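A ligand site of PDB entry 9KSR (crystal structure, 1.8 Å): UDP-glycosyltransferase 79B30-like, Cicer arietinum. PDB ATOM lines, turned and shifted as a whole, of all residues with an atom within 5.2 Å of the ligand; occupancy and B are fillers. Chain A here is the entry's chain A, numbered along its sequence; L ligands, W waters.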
ATOM      1  N   TRP A  10       1.412 -20.343 -20.665  1.00  0.00           N
ATOM      2  CA  TRP A  10       0.867 -19.701 -19.470  1.00  0.00           C
ATOM      3  C   TRP A  10       0.346 -18.313 -19.808  1.00  0.00           C
ATOM      4  O   TRP A  10       0.780 -17.657 -20.768  1.00  0.00           O
ATOM      5  CB  TRP A  10       1.958 -19.692 -18.393  1.00  0.00           C
ATOM      6  CG  TRP A  10       1.866 -18.767 -17.188  1.00  0.00           C
ATOM      7  CD1 TRP A  10       2.815 -17.864 -16.786  1.00  0.00           C
ATOM      8  CD2 TRP A  10       0.833 -18.727 -16.191  1.00  0.00           C
ATOM      9  NE1 TRP A  10       2.436 -17.239 -15.631  1.00  0.00           N
ATOM     10  CE2 TRP A  10       1.218 -17.748 -15.236  1.00  0.00           C
ATOM     11  CE3 TRP A  10      -0.392 -19.393 -16.024  1.00  0.00           C
ATOM     12  CZ2 TRP A  10       0.428 -17.434 -14.122  1.00  0.00           C
ATOM     13  CZ3 TRP A  10      -1.180 -19.069 -14.909  1.00  0.00           C
ATOM     14  CH2 TRP A  10      -0.759 -18.095 -13.981  1.00  0.00           C
ATOM     15  N   ALA A  12       0.495 -15.112 -19.507  1.00  0.00           N
ATOM     16  CA  ALA A  12       1.404 -14.036 -19.142  1.00  0.00           C
ATOM     17  C   ALA A  12       2.034 -13.516 -20.424  1.00  0.00           C
ATOM     18  O   ALA A  12       2.386 -14.317 -21.295  1.00  0.00           O
ATOM     19  CB  ALA A  12       2.496 -14.519 -18.173  1.00  0.00           C
ATOM     20  N   HIS A  15       5.269 -15.061 -21.587  1.00  0.00           N
ATOM     21  CA  HIS A  15       5.196 -16.371 -22.230  1.00  0.00           C
ATOM     22  C   HIS A  15       4.513 -16.282 -23.582  1.00  0.00           C
ATOM     23  O   HIS A  15       4.994 -16.875 -24.557  1.00  0.00           O
ATOM     24  CB  HIS A  15       4.456 -17.376 -21.323  1.00  0.00           C
ATOM     25  CG  HIS A  15       5.175 -17.659 -20.046  1.00  0.00           C
ATOM     26  ND1 HIS A  15       5.549 -18.932 -19.662  1.00  0.00           N
ATOM     27  CD2 HIS A  15       5.611 -16.834 -19.064  1.00  0.00           C
ATOM     28  CE1 HIS A  15       6.170 -18.875 -18.500  1.00  0.00           C
ATOM     29  NE2 HIS A  15       6.226 -17.606 -18.123  1.00  0.00           N
ATOM     30  N   THR A  75      -1.236 -12.408 -16.208  1.00  0.00           N
ATOM     31  CA  THR A  75      -0.577 -11.807 -15.051  1.00  0.00           C
ATOM     32  C   THR A  75      -0.374 -10.307 -15.197  1.00  0.00           C
ATOM     33  O   THR A  75      -0.066  -9.643 -14.208  1.00  0.00           O
ATOM     34  CB  THR A  75       0.775 -12.476 -14.777  1.00  0.00           C
ATOM     35  OG1 THR A  75       1.605 -12.326 -15.925  1.00  0.00           O
ATOM     36  CG2 THR A  75       0.609 -13.953 -14.452  1.00  0.00           C
ATOM     37  N   ILE A  80       0.685  -9.836  -8.291  1.00  0.00           N
ATOM     38  CA  ILE A  80       1.468 -11.070  -8.238  1.00  0.00           C
ATOM     39  C   ILE A  80       0.862 -12.054  -7.240  1.00  0.00           C
ATOM     40  O   ILE A  80       0.927 -13.274  -7.449  1.00  0.00           O
ATOM     41  CB  ILE A  80       2.940 -10.754  -7.931  1.00  0.00           C
ATOM     42  CG1 ILE A  80       3.779 -12.003  -8.114  1.00  0.00           C
ATOM     43  CG2 ILE A  80       3.092 -10.212  -6.509  1.00  0.00           C
ATOM     44  CD1 ILE A  80       4.194 -12.197  -9.570  1.00  0.00           C
ATOM     45  N   PHE A 111       3.356 -26.619 -24.088  1.00  0.00           N
ATOM     46  CA  PHE A 111       2.577 -26.135 -22.960  1.00  0.00           C
ATOM     47  C   PHE A 111       3.459 -25.687 -21.795  1.00  0.00           C
ATOM     48  O   PHE A 111       4.632 -26.047 -21.705  1.00  0.00           O
ATOM     49  CB  PHE A 111       1.581 -27.220 -22.464  1.00  0.00           C
ATOM     50  CG  PHE A 111       2.233 -28.336 -21.675  1.00  0.00           C
ATOM     51  CD1 PHE A 111       2.885 -29.367 -22.334  1.00  0.00           C
ATOM     52  CD2 PHE A 111       2.168 -28.373 -20.291  1.00  0.00           C
ATOM     53  CE1 PHE A 111       3.494 -30.398 -21.631  1.00  0.00           C
ATOM     54  CE2 PHE A 111       2.757 -29.411 -19.575  1.00  0.00           C
ATOM     55  CZ  PHE A 111       3.430 -30.425 -20.246  1.00  0.00           C
ATOM     56  N   ASP A 112       2.818 -24.918 -20.897  1.00  0.00           N
ATOM     57  CA  ASP A 112       3.318 -24.512 -19.589  1.00  0.00           C
ATOM     58  C   ASP A 112       2.439 -25.116 -18.517  1.00  0.00           C
ATOM     59  O   ASP A 112       1.218 -25.190 -18.691  1.00  0.00           O
ATOM     60  CB  ASP A 112       3.241 -22.973 -19.398  1.00  0.00           C
ATOM     61  CG  ASP A 112       4.392 -22.223 -20.033  1.00  0.00           C
ATOM     62  OD1 ASP A 112       5.564 -22.639 -19.847  1.00  0.00           O
ATOM     63  OD2 ASP A 112       4.120 -21.184 -20.702  1.00  0.00           O
ATOM     64  N   PHE A 113       3.041 -25.501 -17.384  1.00  0.00           N
ATOM     65  CA  PHE A 113       2.333 -25.630 -16.102  1.00  0.00           C
ATOM     66  C   PHE A 113       1.241 -26.706 -15.956  1.00  0.00           C
ATOM     67  O   PHE A 113       1.028 -27.198 -14.845  1.00  0.00           O
ATOM     68  CB  PHE A 113       1.689 -24.286 -15.730  1.00  0.00           C
ATOM     69  CG  PHE A 113       2.627 -23.274 -15.101  1.00  0.00           C
ATOM     70  CD1 PHE A 113       3.495 -23.609 -14.080  1.00  0.00           C
ATOM     71  CD2 PHE A 113       2.566 -21.943 -15.514  1.00  0.00           C
ATOM     72  CE1 PHE A 113       4.307 -22.633 -13.484  1.00  0.00           C
ATOM     73  CE2 PHE A 113       3.363 -20.974 -14.936  1.00  0.00           C
ATOM     74  CZ  PHE A 113       4.238 -21.319 -13.927  1.00  0.00           C
ATOM     75  N   LEU A 130       6.722 -29.891 -23.014  1.00  0.00           N
ATOM     76  CA  LEU A 130       6.787 -28.837 -22.017  1.00  0.00           C
ATOM     77  C   LEU A 130       7.818 -27.821 -22.485  1.00  0.00           C
ATOM     78  O   LEU A 130       9.010 -28.125 -22.515  1.00  0.00           O
ATOM     79  CB  LEU A 130       7.133 -29.455 -20.668  1.00  0.00           C
ATOM     80  CG  LEU A 130       7.391 -28.553 -19.444  1.00  0.00           C
ATOM     81  CD1 LEU A 130       6.123 -27.777 -19.090  1.00  0.00           C
ATOM     82  CD2 LEU A 130       7.817 -29.418 -18.275  1.00  0.00           C
ATOM     83  N   PHE A 132       9.692 -24.278 -22.039  1.00  0.00           N
ATOM     84  CA  PHE A 132      10.038 -23.210 -21.099  1.00  0.00           C
ATOM     85  C   PHE A 132      10.667 -22.023 -21.828  1.00  0.00           C
ATOM     86  O   PHE A 132      11.601 -22.211 -22.618  1.00  0.00           O
ATOM     87  CB  PHE A 132      11.050 -23.693 -20.056  1.00  0.00           C
ATOM     88  CG  PHE A 132      10.538 -24.724 -19.068  1.00  0.00           C
ATOM     89  CD1 PHE A 132       9.853 -24.331 -17.903  1.00  0.00           C
ATOM     90  CD2 PHE A 132      10.803 -26.073 -19.253  1.00  0.00           C
ATOM     91  CE1 PHE A 132       9.414 -25.290 -16.972  1.00  0.00           C
ATOM     92  CE2 PHE A 132      10.402 -27.028 -18.338  1.00  0.00           C
ATOM     93  CZ  PHE A 132       9.703 -26.651 -17.183  1.00  0.00           C
ATOM     94  N   ILE A 133      10.206 -20.810 -21.520  1.00  0.00           N
ATOM     95  CA  ILE A 133      10.947 -19.623 -21.931  1.00  0.00           C
ATOM     96  C   ILE A 133      11.734 -19.006 -20.764  1.00  0.00           C
ATOM     97  O   ILE A 133      12.300 -17.916 -20.920  1.00  0.00           O
ATOM     98  CB  ILE A 133      10.013 -18.597 -22.600  1.00  0.00           C
ATOM     99  CG1 ILE A 133       8.772 -18.298 -21.736  1.00  0.00           C
ATOM    100  CG2 ILE A 133       9.512 -19.196 -23.906  1.00  0.00           C
ATOM    101  CD1 ILE A 133       9.019 -17.422 -20.543  1.00  0.00           C
ATOM    102  N   ILE A 134      11.785 -19.680 -19.615  1.00  0.00           N
ATOM    103  CA  ILE A 134      12.678 -19.259 -18.535  1.00  0.00           C
ATOM    104  C   ILE A 134      13.996 -20.005 -18.701  1.00  0.00           C
ATOM    105  O   ILE A 134      14.139 -20.858 -19.592  1.00  0.00           O
ATOM    106  CB  ILE A 134      12.069 -19.535 -17.142  1.00  0.00           C
ATOM    107  CG1 ILE A 134      11.749 -21.027 -16.965  1.00  0.00           C
ATOM    108  CG2 ILE A 134      10.822 -18.674 -16.916  1.00  0.00           C
ATOM    109  CD1 ILE A 134      11.577 -21.427 -15.496  1.00  0.00           C
ATOM    110  N   THR A 138      17.483 -22.274 -14.097  1.00  0.00           N
ATOM    111  CA  THR A 138      16.554 -22.108 -12.993  1.00  0.00           C
ATOM    112  C   THR A 138      15.859 -23.419 -12.663  1.00  0.00           C
ATOM    113  O   THR A 138      15.867 -23.873 -11.505  1.00  0.00           O
ATOM    114  CB  THR A 138      15.534 -21.015 -13.355  1.00  0.00           C
ATOM    115  OG1 THR A 138      16.223 -19.787 -13.641  1.00  0.00           O
ATOM    116  CG2 THR A 138      14.568 -20.782 -12.229  1.00  0.00           C
ATOM    117  N   ILE A 139      15.273 -24.074 -13.664  1.00  0.00           N
ATOM    118  CA  ILE A 139      14.604 -25.363 -13.439  1.00  0.00           C
ATOM    119  C   ILE A 139      15.581 -26.379 -12.878  1.00  0.00           C
ATOM    120  O   ILE A 139      15.241 -27.151 -11.967  1.00  0.00           O
ATOM    121  CB  ILE A 139      13.946 -25.852 -14.748  1.00  0.00           C
ATOM    122  CG1 ILE A 139      12.752 -24.963 -15.089  1.00  0.00           C
ATOM    123  CG2 ILE A 139      13.538 -27.342 -14.658  1.00  0.00           C
ATOM    124  CD1 ILE A 139      11.618 -24.992 -14.020  1.00  0.00           C
ATOM    125  N   THR A 142      16.204 -25.714  -9.008  1.00  0.00           N
ATOM    126  CA  THR A 142      15.119 -25.787  -8.023  1.00  0.00           C
ATOM    127  C   THR A 142      14.236 -27.013  -8.172  1.00  0.00           C
ATOM    128  O   THR A 142      13.533 -27.356  -7.218  1.00  0.00           O
ATOM    129  CB  THR A 142      14.219 -24.558  -8.148  1.00  0.00           C
ATOM    130  OG1 THR A 142      13.650 -24.574  -9.458  1.00  0.00           O
ATOM    131  CG2 THR A 142      15.006 -23.255  -7.975  1.00  0.00           C
ATOM    132  N   THR A 143      14.207 -27.644  -9.349  1.00  0.00           N
ATOM    133  CA  THR A 143      13.161 -28.595  -9.678  1.00  0.00           C
ATOM    134  C   THR A 143      13.755 -29.887 -10.250  1.00  0.00           C
ATOM    135  O   THR A 143      13.010 -30.727 -10.774  1.00  0.00           O
ATOM    136  CB  THR A 143      12.137 -27.951 -10.653  1.00  0.00           C
ATOM    137  OG1 THR A 143      11.903 -26.580 -10.267  1.00  0.00           O
ATOM    138  CG2 THR A 143      10.757 -28.691 -10.639  1.00  0.00           C
ATOM    139  N   LEU A 180      13.418 -18.779  -2.095  1.00  0.00           N
ATOM    140  CA  LEU A 180      13.214 -20.039  -2.823  1.00  0.00           C
ATOM    141  C   LEU A 180      12.740 -21.145  -1.889  1.00  0.00           C
ATOM    142  O   LEU A 180      11.908 -21.977  -2.285  1.00  0.00           O
ATOM    143  CB  LEU A 180      14.499 -20.449  -3.522  1.00  0.00           C
ATOM    144  CG  LEU A 180      15.036 -19.557  -4.640  1.00  0.00           C
ATOM    145  CD1 LEU A 180      16.339 -20.153  -5.186  1.00  0.00           C
ATOM    146  CD2 LEU A 180      14.019 -19.393  -5.753  1.00  0.00           C
ATOM    147  N   PHE A 188       0.249 -23.154  -5.976  1.00  0.00           N
ATOM    148  CA  PHE A 188       0.139 -22.372  -7.207  1.00  0.00           C
ATOM    149  C   PHE A 188      -0.888 -23.077  -8.087  1.00  0.00           C
ATOM    150  O   PHE A 188      -0.526 -23.869  -8.969  1.00  0.00           O
ATOM    151  CB  PHE A 188       1.506 -22.237  -7.899  1.00  0.00           C
ATOM    152  CG  PHE A 188       1.508 -21.286  -9.061  1.00  0.00           C
ATOM    153  CD1 PHE A 188       1.395 -19.915  -8.859  1.00  0.00           C
ATOM    154  CD2 PHE A 188       1.608 -21.760 -10.357  1.00  0.00           C
ATOM    155  CE1 PHE A 188       1.411 -19.022  -9.949  1.00  0.00           C
ATOM    156  CE2 PHE A 188       1.621 -20.898 -11.439  1.00  0.00           C
ATOM    157  CZ  PHE A 188       1.500 -19.515 -11.234  1.00  0.00           C
ATOM    158  N   PHE A 194       3.977 -25.116  -5.685  1.00  0.00           N
ATOM    159  CA  PHE A 194       4.578 -24.584  -6.909  1.00  0.00           C
ATOM    160  C   PHE A 194       5.603 -25.544  -7.514  1.00  0.00           C
ATOM    161  O   PHE A 194       5.517 -25.900  -8.695  1.00  0.00           O
ATOM    162  CB  PHE A 194       5.182 -23.205  -6.626  1.00  0.00           C
ATOM    163  CG  PHE A 194       5.803 -22.565  -7.844  1.00  0.00           C
ATOM    164  CD1 PHE A 194       5.008 -21.983  -8.803  1.00  0.00           C
ATOM    165  CD2 PHE A 194       7.182 -22.489  -7.982  1.00  0.00           C
ATOM    166  CE1 PHE A 194       5.550 -21.366  -9.928  1.00  0.00           C
ATOM    167  CE2 PHE A 194       7.748 -21.867  -9.090  1.00  0.00           C
ATOM    168  CZ  PHE A 194       6.925 -21.309 -10.067  1.00  0.00           C
ATOM    169  N   SER A 195       6.596 -25.977  -6.728  1.00  0.00           N
ATOM    170  CA  SER A 195       7.627 -26.804  -7.361  1.00  0.00           C
ATOM    171  C   SER A 195       7.090 -28.191  -7.718  1.00  0.00           C
ATOM    172  O   SER A 195       7.506 -28.770  -8.722  1.00  0.00           O
ATOM    173  CB  SER A 195       8.873 -26.892  -6.473  1.00  0.00           C
ATOM    174  OG  SER A 195       9.532 -25.631  -6.395  1.00  0.00           O
ATOM    175  N   SER A 198       5.623 -28.011 -11.291  1.00  0.00           N
ATOM    176  CA  SER A 198       6.576 -28.050 -12.386  1.00  0.00           C
ATOM    177  C   SER A 198       7.249 -29.407 -12.479  1.00  0.00           C
ATOM    178  O   SER A 198       7.573 -29.883 -13.569  1.00  0.00           O
ATOM    179  CB  SER A 198       7.636 -26.958 -12.219  1.00  0.00           C
ATOM    180  OG  SER A 198       7.079 -25.681 -12.480  1.00  0.00           O
ATOM    181  N   CYS A 201       5.012 -31.677 -14.289  1.00  0.00           N
ATOM    182  CA  CYS A 201       5.103 -31.427 -15.728  1.00  0.00           C
ATOM    183  C   CYS A 201       6.335 -32.088 -16.319  1.00  0.00           C
ATOM    184  O   CYS A 201       6.242 -32.811 -17.320  1.00  0.00           O
ATOM    185  CB  CYS A 201       5.110 -29.932 -16.034  1.00  0.00           C
ATOM    186  SG  CYS A 201       3.564 -29.075 -15.696  1.00  0.00           S
ATOM    187  N   GLU A 271       4.556  -7.541 -14.700  1.00  0.00           N
ATOM    188  CA  GLU A 271       3.867  -8.308 -13.676  1.00  0.00           C
ATOM    189  C   GLU A 271       4.047  -7.759 -12.278  1.00  0.00           C
ATOM    190  O   GLU A 271       3.384  -8.260 -11.356  1.00  0.00           O
ATOM    191  CB  GLU A 271       4.356  -9.760 -13.675  1.00  0.00           C
ATOM    192  CG  GLU A 271       4.217 -10.518 -14.947  1.00  0.00           C
ATOM    193  CD  GLU A 271       4.724 -11.934 -14.772  1.00  0.00           C
ATOM    194  OE1 GLU A 271       5.877 -12.079 -14.322  1.00  0.00           O
ATOM    195  OE2 GLU A 271       3.957 -12.878 -15.047  1.00  0.00           O
ATOM    196  N   ASN A 369      12.530 -13.367  -7.580  1.00  0.00           N
ATOM    197  CA  ASN A 369      11.987 -14.437  -8.414  1.00  0.00           C
ATOM    198  C   ASN A 369      13.197 -15.270  -8.804  1.00  0.00           C
ATOM    199  O   ASN A 369      14.226 -14.699  -9.161  1.00  0.00           O
ATOM    200  CB  ASN A 369      11.292 -13.825  -9.642  1.00  0.00           C
ATOM    201  CG  ASN A 369      10.957 -14.844 -10.732  1.00  0.00           C
ATOM    202  OD1 ASN A 369      11.844 -15.367 -11.414  1.00  0.00           O
ATOM    203  ND2 ASN A 369       9.664 -15.013 -10.985  1.00  0.00           N
ATOM    204  N   GLY A 370      13.077 -16.600  -8.697  1.00  0.00           N
ATOM    205  CA  GLY A 370      14.221 -17.470  -8.967  1.00  0.00           C
ATOM    206  C   GLY A 370      14.827 -17.286 -10.348  1.00  0.00           C
ATOM    207  O   GLY A 370      16.052 -17.262 -10.496  1.00  0.00           O
ATOM    208  N   ASP A 371      13.984 -17.158 -11.383  1.00  0.00           N
ATOM    209  CA  ASP A 371      14.545 -16.979 -12.727  1.00  0.00           C
ATOM    210  C   ASP A 371      15.260 -15.632 -12.863  1.00  0.00           C
ATOM    211  O   ASP A 371      16.330 -15.560 -13.489  1.00  0.00           O
ATOM    212  CB  ASP A 371      13.473 -17.113 -13.809  1.00  0.00           C
ATOM    213  CG  ASP A 371      14.086 -17.377 -15.193  1.00  0.00           C
ATOM    214  OD1 ASP A 371      14.822 -18.377 -15.324  1.00  0.00           O
ATOM    215  OD2 ASP A 371      13.832 -16.598 -16.145  1.00  0.00           O
HETATM  216  C1  LIG L   1       4.842 -16.439 -12.819  1.00  0.00           C
HETATM  217  C2  LIG L   1       5.828 -17.153 -11.926  1.00  0.00           C
HETATM  218  C3  LIG L   1       5.172 -17.726 -10.686  1.00  0.00           C
HETATM  219  C4  LIG L   1       5.503 -15.965 -14.111  1.00  0.00           C
HETATM  220  C5  LIG L   1       7.374 -23.132 -14.447  1.00  0.00           C
HETATM  221  C6  LIG L   1       6.698 -23.886 -15.392  1.00  0.00           C
HETATM  222  O1  LIG L   1       6.338 -25.183 -15.107  1.00  0.00           O
HETATM  223  C7  LIG L   1       6.383 -23.331 -16.629  1.00  0.00           C
HETATM  224  O2  LIG L   1       5.748 -24.114 -17.553  1.00  0.00           O
HETATM  225  C8  LIG L   1       6.735 -22.022 -16.911  1.00  0.00           C
HETATM  226  C9  LIG L   1       7.412 -21.269 -15.957  1.00  0.00           C
HETATM  227  C10 LIG L   1       7.696 -21.789 -14.700  1.00  0.00           C
HETATM  228  C11 LIG L   1       8.462 -21.044 -13.700  1.00  0.00           C
HETATM  229  O3  LIG L   1       9.152 -21.875 -12.859  1.00  0.00           O
HETATM  230  C12 LIG L   1       9.963 -21.402 -11.873  1.00  0.00           C
HETATM  231  C13 LIG L   1      10.551 -22.365 -11.068  1.00  0.00           C
HETATM  232  C14 LIG L   1      11.377 -21.897 -10.054  1.00  0.00           C
HETATM  233  O4  LIG L   1      11.937 -22.805  -9.228  1.00  0.00           O
HETATM  234  C15 LIG L   1      11.632 -20.530  -9.865  1.00  0.00           C
HETATM  235  C16 LIG L   1      11.031 -19.615 -10.693  1.00  0.00           C
HETATM  236  O5  LIG L   1      11.277 -18.296 -10.507  1.00  0.00           O
HETATM  237  C17 LIG L   1      10.168 -20.034 -11.726  1.00  0.00           C
HETATM  238  C18 LIG L   1       9.478 -19.138 -12.632  1.00  0.00           C
HETATM  239  O6  LIG L   1       9.660 -17.893 -12.554  1.00  0.00           O
HETATM  240  C19 LIG L   1       8.636 -19.677 -13.609  1.00  0.00           C
HETATM  241  O7  LIG L   1       7.923 -18.823 -14.434  1.00  0.00           O
HETATM  242  C20 LIG L   1       7.179 -17.785 -13.778  1.00  0.00           C
HETATM  243  O8  LIG L   1       6.433 -18.252 -12.666  1.00  0.00           O
HETATM  244  O9  LIG L   1       6.117 -18.023  -9.674  1.00  0.00           O
HETATM  245  O10 LIG L   1       4.320 -15.324 -12.092  1.00  0.00           O
HETATM  246  O11 LIG L   1       4.496 -15.452 -14.989  1.00  0.00           O
HETATM  247  C21 LIG L   1       6.276 -17.109 -14.792  1.00  0.00           C
HETATM  248  O12 LIG L   1       7.073 -16.622 -15.871  1.00  0.00           O
HETATM  249  O   HOH W   1       6.151 -13.006 -11.931  1.00  0.00           O
HETATM  250  O   HOH W   2      10.146 -25.013  -8.836  1.00  0.00           O
HETATM  251  O   HOH W   3      10.550 -17.552  -7.416  1.00  0.00           O
HETATM  252  O   HOH W   4       6.360 -13.936 -17.009  1.00  0.00           O
HETATM  253  O   HOH W   5       7.274 -18.982  -6.887  1.00  0.00           O
HETATM  254  O   HOH W   6      11.284 -22.375  -6.669  1.00  0.00           O
HETATM  255  O   HOH W   7       8.292 -16.276  -8.108  1.00  0.00           O
HETATM  256  O   HOH W   8       1.850 -15.095 -11.279  1.00  0.00           O
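An oxygen (O5) of the ligand sits at hydrogen-bond distance from the backbone NH (N) of Asp 371, 3.1 Å away.
The side-chain hydroxyl (OG1) of Thr 142 sits at hydrogen-bond distance from an oxygen (O4) of the ligand, at 2.5 Å.
The backbone NH (N) of Gly 370 is in hydrogen-bond range of an oxygen (O5) of the ligand, 3.1 Å away.
NE2 of His 15 sits at hydrogen-bond distance from O12 of the ligand (2.6 Å).
An oxygen (O2) of the ligand lies within hydrogen-bond range of the side-chain carboxylate (OD1) of Asp 112, 2.7 Å away.
NE1 of Trp 10 sits at hydrogen-bond distance from O11 of the ligand, 2.8 Å away.
O11 of the ligand sits at hydrogen-bond distance from OE2 of Glu 271 (2.6 Å).
The side-chain amide oxygen of Asn 369 sits at hydrogen-bond distance from an oxygen (O5) of the ligand, at 3.1 Å.
The backbone NH (N) of Phe 113 is in hydrogen-bond range of an oxygen (O2) of the ligand, at 3.0 Å.
An oxygen (O1) of the ligand lies within hydrogen-bond range of the side-chain hydroxyl (OG) of Ser 198, 2.8 Å away.
The backbone carbonyl oxygen (O) of Thr 138 is in hydrogen-bond range of the side-chain hydroxyl (OG1) of Thr 142 (3.1 Å).
The side-chain hydroxyl (OG1) of Thr 142 lies within hydrogen-bond range of the side-chain hydroxyl (OG1) of Thr 143 (2.8 Å).
The backbone NH of Asp 371 sits at hydrogen-bond distance from the side-chain amide oxygen of Asn 369 (2.8 Å).
A ring nitrogen (ND1) of His 15 is in hydrogen-bond range of the side-chain carboxylate (OD2) of Asp 112 (2.9 Å).
The side-chain hydroxyl of Thr 75 is in hydrogen-bond range of the side-chain carboxylate of Glu 271, 2.6 Å away.
The side-chain sulfur of Cys 201 lies within hydrogen-bond range of the backbone carbonyl oxygen of Phe 113 (3.3 Å).
N of Trp 10 lies within hydrogen-bond range of OD2 of Asp 112, 2.8 Å away.
The side-chain hydroxyl (OG1) of Thr 138 is in hydrogen-bond range of the side-chain carboxylate (OD1) of Asp 371, 2.6 Å away.
Water W2 lies within hydrogen-bond range of OG of Ser 195 (2.6 Å), OG1 of Thr 143 (2.8 Å) and O4 of the ligand (2.9 Å).
Water W1 lies within hydrogen-bond range of OE1 of Glu 271 (2.6 Å) and O10 of the ligand (3.0 Å).
Water W4 bridges an oxygen (O12) of the ligand and the side-chain carboxylate of Glu 271.
Water W7 bridges O9 of the ligand (3.2 Å) and ND2 of Asn 369 (3.4 Å).
Water W3 lies within hydrogen-bond range of N of Gly 370 (3.0 Å) and O5 of the ligand (3.3 Å).
Residues that only touch the ligand: Phe 194 (3.4 Å), Phe 132 (3.4 Å), Ile 134 (3.6 Å), Thr 138 (3.8 Å), Ala 12 (3.9 Å), Thr 143 (3.9 Å) and Leu 130 (3.99 Å).
Hydrophobic or aromatic side chains within 4 Å of the ligand: Trp 10, Ala 12, His 15, Phe 113, Leu 130, Phe 132, Ile 134 and Phe 194.
Of the 26 residues printed, 17 come within 4 Å of the ligand.
Along chain A the residues within 4 Å of the ligand span positions 10 to 371.
The nearest printed residue that does not touch the ligand is Ile 80 (4.02 Å).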
